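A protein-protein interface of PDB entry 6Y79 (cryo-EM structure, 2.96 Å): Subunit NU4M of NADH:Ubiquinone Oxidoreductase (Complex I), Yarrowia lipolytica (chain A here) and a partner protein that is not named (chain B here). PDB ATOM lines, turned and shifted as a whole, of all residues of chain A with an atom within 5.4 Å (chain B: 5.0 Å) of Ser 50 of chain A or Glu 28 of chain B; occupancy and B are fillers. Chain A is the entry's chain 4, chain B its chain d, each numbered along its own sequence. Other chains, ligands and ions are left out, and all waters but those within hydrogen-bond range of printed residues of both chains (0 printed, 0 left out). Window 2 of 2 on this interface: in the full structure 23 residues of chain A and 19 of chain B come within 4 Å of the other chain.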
ATOM      1  N   PHE A  46      32.843  11.973   4.075  1.00  0.00           N
ATOM      2  CA  PHE A  46      31.600  12.719   3.955  1.00  0.00           C
ATOM      3  C   PHE A  46      30.844  12.287   2.704  1.00  0.00           C
ATOM      4  O   PHE A  46      31.429  12.172   1.625  1.00  0.00           O
ATOM      5  CB  PHE A  46      31.910  14.215   3.916  1.00  0.00           C
ATOM      6  CG  PHE A  46      30.704  15.093   3.842  1.00  0.00           C
ATOM      7  CD1 PHE A  46      29.998  15.411   4.980  1.00  0.00           C
ATOM      8  CD2 PHE A  46      30.295  15.629   2.635  1.00  0.00           C
ATOM      9  CE1 PHE A  46      28.900  16.224   4.915  1.00  0.00           C
ATOM     10  CE2 PHE A  46      29.185  16.437   2.564  1.00  0.00           C
ATOM     11  CZ  PHE A  46      28.487  16.733   3.706  1.00  0.00           C
ATOM     12  N   ASN A  47      29.546  12.052   2.846  1.00  0.00           N
ATOM     13  CA  ASN A  47      28.697  11.687   1.720  1.00  0.00           C
ATOM     14  C   ASN A  47      28.076  12.947   1.136  1.00  0.00           C
ATOM     15  O   ASN A  47      27.234  13.582   1.775  1.00  0.00           O
ATOM     16  CB  ASN A  47      27.607  10.709   2.151  1.00  0.00           C
ATOM     17  CG  ASN A  47      26.893  10.069   0.973  1.00  0.00           C
ATOM     18  OD1 ASN A  47      27.258  10.268  -0.179  1.00  0.00           O
ATOM     19  ND2 ASN A  47      25.860   9.302   1.264  1.00  0.00           N
ATOM     20  N   THR A  48      28.479  13.296  -0.082  1.00  0.00           N
ATOM     21  CA  THR A  48      27.937  14.475  -0.735  1.00  0.00           C
ATOM     22  C   THR A  48      26.590  14.212  -1.383  1.00  0.00           C
ATOM     23  O   THR A  48      25.864  15.164  -1.683  1.00  0.00           O
ATOM     24  CB  THR A  48      28.921  14.985  -1.783  1.00  0.00           C
ATOM     25  OG1 THR A  48      29.032  14.022  -2.835  1.00  0.00           O
ATOM     26  CG2 THR A  48      30.284  15.195  -1.161  1.00  0.00           C
ATOM     27  N   PHE A  49      26.233  12.947  -1.587  1.00  0.00           N
ATOM     28  CA  PHE A  49      24.976  12.583  -2.226  1.00  0.00           C
ATOM     29  C   PHE A  49      23.796  12.605  -1.266  1.00  0.00           C
ATOM     30  O   PHE A  49      22.672  12.306  -1.679  1.00  0.00           O
ATOM     31  CB  PHE A  49      25.111  11.202  -2.866  1.00  0.00           C
ATOM     32  CG  PHE A  49      24.157  10.960  -3.994  1.00  0.00           C
ATOM     33  CD1 PHE A  49      24.208  11.732  -5.138  1.00  0.00           C
ATOM     34  CD2 PHE A  49      23.205   9.962  -3.906  1.00  0.00           C
ATOM     35  CE1 PHE A  49      23.329  11.513  -6.174  1.00  0.00           C
ATOM     36  CE2 PHE A  49      22.323   9.738  -4.943  1.00  0.00           C
ATOM     37  CZ  PHE A  49      22.387  10.515  -6.076  1.00  0.00           C
ATOM     38  N   SER A  50      24.012  12.965  -0.008  1.00  0.00           N
ATOM     39  CA  SER A  50      22.958  13.011   0.992  1.00  0.00           C
ATOM     40  C   SER A  50      22.769  14.438   1.483  1.00  0.00           C
ATOM     41  O   SER A  50      23.740  15.111   1.841  1.00  0.00           O
ATOM     42  CB  SER A  50      23.282  12.093   2.168  1.00  0.00           C
ATOM     43  OG  SER A  50      22.257  12.150   3.138  1.00  0.00           O
ATOM     44  N   ASN A  51      21.517  14.892   1.496  1.00  0.00           N
ATOM     45  CA  ASN A  51      21.173  16.190   2.057  1.00  0.00           C
ATOM     46  C   ASN A  51      21.224  16.192   3.579  1.00  0.00           C
ATOM     47  O   ASN A  51      21.355  17.260   4.182  1.00  0.00           O
ATOM     48  CB  ASN A  51      19.775  16.577   1.580  1.00  0.00           C
ATOM     49  CG  ASN A  51      19.468  18.045   1.763  1.00  0.00           C
ATOM     50  OD1 ASN A  51      20.344  18.855   2.060  1.00  0.00           O
ATOM     51  ND2 ASN A  51      18.201  18.397   1.588  1.00  0.00           N
ATOM     52  N   SER A  52      21.137  15.024   4.208  1.00  0.00           N
ATOM     53  CA  SER A  52      20.985  14.926   5.651  1.00  0.00           C
ATOM     54  C   SER A  52      22.305  15.209   6.369  1.00  0.00           C
ATOM     55  O   SER A  52      23.346  15.442   5.754  1.00  0.00           O
ATOM     56  CB  SER A  52      20.447  13.545   6.028  1.00  0.00           C
ATOM     57  OG  SER A  52      21.381  12.541   5.720  1.00  0.00           O
ATOM     58  N   GLN A  54      25.418  14.236   8.613  1.00  0.00           N
ATOM     59  CA  GLN A  54      26.129  12.964   8.543  1.00  0.00           C
ATOM     60  C   GLN A  54      26.758  12.534   9.861  1.00  0.00           C
ATOM     61  O   GLN A  54      26.610  11.373  10.260  1.00  0.00           O
ATOM     62  CB  GLN A  54      27.207  13.015   7.456  1.00  0.00           C
ATOM     63  CG  GLN A  54      26.697  12.810   6.048  1.00  0.00           C
ATOM     64  CD  GLN A  54      26.132  14.073   5.463  1.00  0.00           C
ATOM     65  OE1 GLN A  54      26.206  15.133   6.075  1.00  0.00           O
ATOM     66  NE2 GLN A  54      25.560  13.976   4.276  1.00  0.00           N
ATOM     67  N   TYR A 476      25.873  22.022  -3.385  1.00  0.00           N
ATOM     68  CA  TYR A 476      24.809  21.952  -4.380  1.00  0.00           C
ATOM     69  C   TYR A 476      23.467  21.566  -3.782  1.00  0.00           C
ATOM     70  O   TYR A 476      22.428  21.879  -4.371  1.00  0.00           O
ATOM     71  CB  TYR A 476      25.185  20.994  -5.513  1.00  0.00           C
ATOM     72  CG  TYR A 476      25.383  19.538  -5.163  1.00  0.00           C
ATOM     73  CD1 TYR A 476      24.314  18.651  -5.134  1.00  0.00           C
ATOM     74  CD2 TYR A 476      26.651  19.035  -4.934  1.00  0.00           C
ATOM     75  CE1 TYR A 476      24.500  17.329  -4.841  1.00  0.00           C
ATOM     76  CE2 TYR A 476      26.845  17.709  -4.645  1.00  0.00           C
ATOM     77  CZ  TYR A 476      25.766  16.862  -4.599  1.00  0.00           C
ATOM     78  OH  TYR A 476      25.954  15.535  -4.311  1.00  0.00           O
ATOM     79  N   TRP A 477      23.462  20.898  -2.632  1.00  0.00           N
ATOM     80  CA  TRP A 477      22.225  20.741  -1.885  1.00  0.00           C
ATOM     81  C   TRP A 477      21.806  22.066  -1.282  1.00  0.00           C
ATOM     82  O   TRP A 477      20.695  22.546  -1.523  1.00  0.00           O
ATOM     83  CB  TRP A 477      22.393  19.695  -0.788  1.00  0.00           C
ATOM     84  CG  TRP A 477      22.622  18.327  -1.286  1.00  0.00           C
ATOM     85  CD1 TRP A 477      23.780  17.631  -1.235  1.00  0.00           C
ATOM     86  CD2 TRP A 477      21.668  17.477  -1.917  1.00  0.00           C
ATOM     87  NE1 TRP A 477      23.613  16.394  -1.793  1.00  0.00           N
ATOM     88  CE2 TRP A 477      22.320  16.276  -2.223  1.00  0.00           C
ATOM     89  CE3 TRP A 477      20.324  17.615  -2.257  1.00  0.00           C
ATOM     90  CZ2 TRP A 477      21.679  15.220  -2.848  1.00  0.00           C
ATOM     91  CZ3 TRP A 477      19.689  16.562  -2.872  1.00  0.00           C
ATOM     92  CH2 TRP A 477      20.365  15.385  -3.166  1.00  0.00           C
ATOM     93  N   ARG B  24      12.527  13.600   3.981  1.00  0.00           N
ATOM     94  CA  ARG B  24      13.865  13.831   3.459  1.00  0.00           C
ATOM     95  C   ARG B  24      14.025  13.260   2.054  1.00  0.00           C
ATOM     96  O   ARG B  24      14.689  13.866   1.201  1.00  0.00           O
ATOM     97  CB  ARG B  24      14.887  13.225   4.411  1.00  0.00           C
ATOM     98  CG  ARG B  24      16.253  13.798   4.251  1.00  0.00           C
ATOM     99  CD  ARG B  24      16.251  15.286   4.474  1.00  0.00           C
ATOM    100  NE  ARG B  24      16.529  15.626   5.860  1.00  0.00           N
ATOM    101  CZ  ARG B  24      16.901  16.832   6.261  1.00  0.00           C
ATOM    102  NH1 ARG B  24      17.046  17.806   5.383  1.00  0.00           N
ATOM    103  NH2 ARG B  24      17.141  17.066   7.535  1.00  0.00           N
ATOM    104  N   GLU B  25      13.379  12.125   1.771  1.00  0.00           N
ATOM    105  CA  GLU B  25      13.453  11.582   0.415  1.00  0.00           C
ATOM    106  C   GLU B  25      12.635  12.396  -0.576  1.00  0.00           C
ATOM    107  O   GLU B  25      13.035  12.529  -1.733  1.00  0.00           O
ATOM    108  CB  GLU B  25      13.021  10.122   0.386  1.00  0.00           C
ATOM    109  CG  GLU B  25      13.865   9.272   1.272  1.00  0.00           C
ATOM    110  CD  GLU B  25      13.747   7.806   0.980  1.00  0.00           C
ATOM    111  OE1 GLU B  25      14.092   7.394  -0.147  1.00  0.00           O
ATOM    112  OE2 GLU B  25      13.303   7.062   1.879  1.00  0.00           O
ATOM    113  N   ALA B  26      11.495  12.945  -0.157  1.00  0.00           N
ATOM    114  CA  ALA B  26      10.701  13.770  -1.064  1.00  0.00           C
ATOM    115  C   ALA B  26      11.421  15.069  -1.380  1.00  0.00           C
ATOM    116  O   ALA B  26      11.384  15.560  -2.517  1.00  0.00           O
ATOM    117  CB  ALA B  26       9.336  14.057  -0.448  1.00  0.00           C
ATOM    118  N   GLN B  27      12.101  15.607  -0.371  1.00  0.00           N
ATOM    119  CA  GLN B  27      12.989  16.756  -0.492  1.00  0.00           C
ATOM    120  C   GLN B  27      14.070  16.524  -1.542  1.00  0.00           C
ATOM    121  O   GLN B  27      14.179  17.270  -2.528  1.00  0.00           O
ATOM    122  CB  GLN B  27      13.586  16.961   0.893  1.00  0.00           C
ATOM    123  CG  GLN B  27      14.255  18.217   1.233  1.00  0.00           C
ATOM    124  CD  GLN B  27      14.449  18.298   2.732  1.00  0.00           C
ATOM    125  OE1 GLN B  27      13.788  17.594   3.486  1.00  0.00           O
ATOM    126  NE2 GLN B  27      15.391  19.115   3.168  1.00  0.00           N
ATOM    127  N   GLU B  28      14.858  15.458  -1.358  1.00  0.00           N
ATOM    128  CA  GLU B  28      15.925  15.136  -2.301  1.00  0.00           C
ATOM    129  C   GLU B  28      15.389  14.752  -3.676  1.00  0.00           C
ATOM    130  O   GLU B  28      16.058  15.001  -4.684  1.00  0.00           O
ATOM    131  CB  GLU B  28      16.787  14.007  -1.749  1.00  0.00           C
ATOM    132  CG  GLU B  28      17.502  14.327  -0.461  1.00  0.00           C
ATOM    133  CD  GLU B  28      18.370  13.177   0.006  1.00  0.00           C
ATOM    134  OE1 GLU B  28      18.326  12.108  -0.635  1.00  0.00           O
ATOM    135  OE2 GLU B  28      19.092  13.330   1.012  1.00  0.00           O
ATOM    136  N   SER B  29      14.190  14.164  -3.737  1.00  0.00           N
ATOM    137  CA  SER B  29      13.588  13.789  -5.010  1.00  0.00           C
ATOM    138  C   SER B  29      13.281  15.015  -5.843  1.00  0.00           C
ATOM    139  O   SER B  29      13.684  15.104  -7.006  1.00  0.00           O
ATOM    140  CB  SER B  29      12.309  12.990  -4.766  1.00  0.00           C
ATOM    141  OG  SER B  29      12.565  11.803  -4.044  1.00  0.00           O
ATOM    142  N   TYR B  30      12.571  15.974  -5.246  1.00  0.00           N
ATOM    143  CA  TYR B  30      12.208  17.216  -5.921  1.00  0.00           C
ATOM    144  C   TYR B  30      13.449  18.005  -6.343  1.00  0.00           C
ATOM    145  O   TYR B  30      13.503  18.561  -7.456  1.00  0.00           O
ATOM    146  CB  TYR B  30      11.318  18.006  -4.966  1.00  0.00           C
ATOM    147  CG  TYR B  30      10.608  19.211  -5.494  1.00  0.00           C
ATOM    148  CD1 TYR B  30       9.371  19.109  -6.104  1.00  0.00           C
ATOM    149  CD2 TYR B  30      11.145  20.462  -5.314  1.00  0.00           C
ATOM    150  CE1 TYR B  30       8.714  20.231  -6.555  1.00  0.00           C
ATOM    151  CE2 TYR B  30      10.500  21.581  -5.751  1.00  0.00           C
ATOM    152  CZ  TYR B  30       9.288  21.465  -6.374  1.00  0.00           C
ATOM    153  OH  TYR B  30       8.656  22.601  -6.814  1.00  0.00           O
ATOM    154  N   THR B  31      14.489  17.976  -5.503  1.00  0.00           N
ATOM    155  CA  THR B  31      15.765  18.614  -5.829  1.00  0.00           C
ATOM    156  C   THR B  31      16.431  17.987  -7.057  1.00  0.00           C
ATOM    157  O   THR B  31      16.772  18.686  -8.028  1.00  0.00           O
ATOM    158  CB  THR B  31      16.678  18.521  -4.607  1.00  0.00           C
ATOM    159  OG1 THR B  31      16.173  19.365  -3.570  1.00  0.00           O
ATOM    160  CG2 THR B  31      18.065  18.942  -4.940  1.00  0.00           C
ATOM    161  N   ARG B  32      16.612  16.659  -7.040  1.00  0.00           N
ATOM    162  CA  ARG B  32      17.271  15.975  -8.149  1.00  0.00           C
ATOM    163  C   ARG B  32      16.462  16.057  -9.436  1.00  0.00           C
ATOM    164  O   ARG B  32      17.040  16.067 -10.529  1.00  0.00           O
ATOM    165  CB  ARG B  32      17.538  14.519  -7.781  1.00  0.00           C
ATOM    166  CG  ARG B  32      18.643  14.337  -6.768  1.00  0.00           C
ATOM    167  CD  ARG B  32      18.862  12.877  -6.421  1.00  0.00           C
ATOM    168  NE  ARG B  32      17.737  12.316  -5.681  1.00  0.00           N
ATOM    169  CZ  ARG B  32      16.911  11.400  -6.169  1.00  0.00           C
ATOM    170  NH1 ARG B  32      15.912  10.943  -5.433  1.00  0.00           N
ATOM    171  NH2 ARG B  32      17.090  10.937  -7.397  1.00  0.00           N
ATOM    172  N   GLU B  33      15.138  16.171  -9.331  1.00  0.00           N
ATOM    173  CA  GLU B  33      14.331  16.343 -10.531  1.00  0.00           C
ATOM    174  C   GLU B  33      14.533  17.717 -11.148  1.00  0.00           C
ATOM    175  O   GLU B  33      14.522  17.858 -12.381  1.00  0.00           O
ATOM    176  CB  GLU B  33      12.854  16.107 -10.222  1.00  0.00           C
ATOM    177  CG  GLU B  33      12.497  14.652  -9.953  1.00  0.00           C
ATOM    178  CD  GLU B  33      13.012  13.726 -11.017  1.00  0.00           C
ATOM    179  OE1 GLU B  33      12.864  14.065 -12.197  1.00  0.00           O
ATOM    180  OE2 GLU B  33      13.581  12.669 -10.686  1.00  0.00           O
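Ser 50 of chain A touches just one residue of chain B: Glu 28 (3.9 Å).
Of the printed residues of chain A, Glu 28 of chain B touches Ser 50 (3.9 Å), Asn 51 (2.9 Å) and Trp 477 (3.9 Å).
Printed residues of chain B within 4 Å of Asn 51 of chain A: Gln 27 and Glu 28.
Of the printed residues of chain A, Thr 31 of chain B touches Trp 477.
Of the printed residues of chain B, Trp 477 of chain A touches Glu 28 and Thr 31.
Printed residues of chain A within 4 Å of Gln 27 of chain B: Asn 51 (3.3 Å).
Asn 47 of chain A touches none of the printed residues of chain B.
The nearest printed residue of chain B that does not touch Ser 50 of chain A is Arg 24 of chain B (6.3 Å).
The nearest residue of chain A that does not touch Glu 28 of chain B is Ser 52 of chain A (4.2 Å).
The guanidinium group of Arg 32 of chain B lies within hydrogen-bond range of the backbone carbonyl oxygen of Glu 28 of chain B.
The side-chain hydroxyl of Ser 50 of chain A sits at hydrogen-bond distance from the side-chain hydroxyl of Ser 52 of chain A (2.8 Å).
O of Ser 50 of chain A lies within hydrogen-bond range of NE2 of Gln 54 of chain A (3.2 Å).
The indole nitrogen of Trp 477 of chain A sits at hydrogen-bond distance from the backbone carbonyl oxygen of Thr 48 of chain A, at 2.6 Å.
The side-chain amide nitrogen (NE2) of Gln 27 of chain B lies close to the guanidinium group (NH1) of Arg 24 of chain B (3.1 Å).
The backbone carbonyl oxygen of Gln 27 of chain B sits at hydrogen-bond distance from the side-chain hydroxyl of Thr 31 of chain B (3.1 Å).
OE2 of Glu 28 of chain B touches C of Ser 50 of chain A (3.9 Å).
Glu 28 of chain B touches Trp 477 of chain A.
CZ3 of Trp 477 of chain A touches CG2 of Thr 31 of chain B, 3.5 Å away.
Of the 10 printed residues of chain B, 3 touch a printed residue of chain A.
Of the 10 printed residues of chain A, 3 touch a printed residue of chain B.
Among the printed residues, 5 pairs touch across the chains.
Among the printed residues, no Asp or Glu carboxylate lies within 4 Å of a Lys or Arg side-chain nitrogen of the other chain.
N of Asn 51 of chain A is in hydrogen-bond range of OE2 of Glu 28 of chain B (2.9 Å).
The side-chain amide nitrogen (NE2) of Gln 27 of chain B lies close to the side-chain amide nitrogen (ND2) of Asn 51 of chain A, at 3.3 Å.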
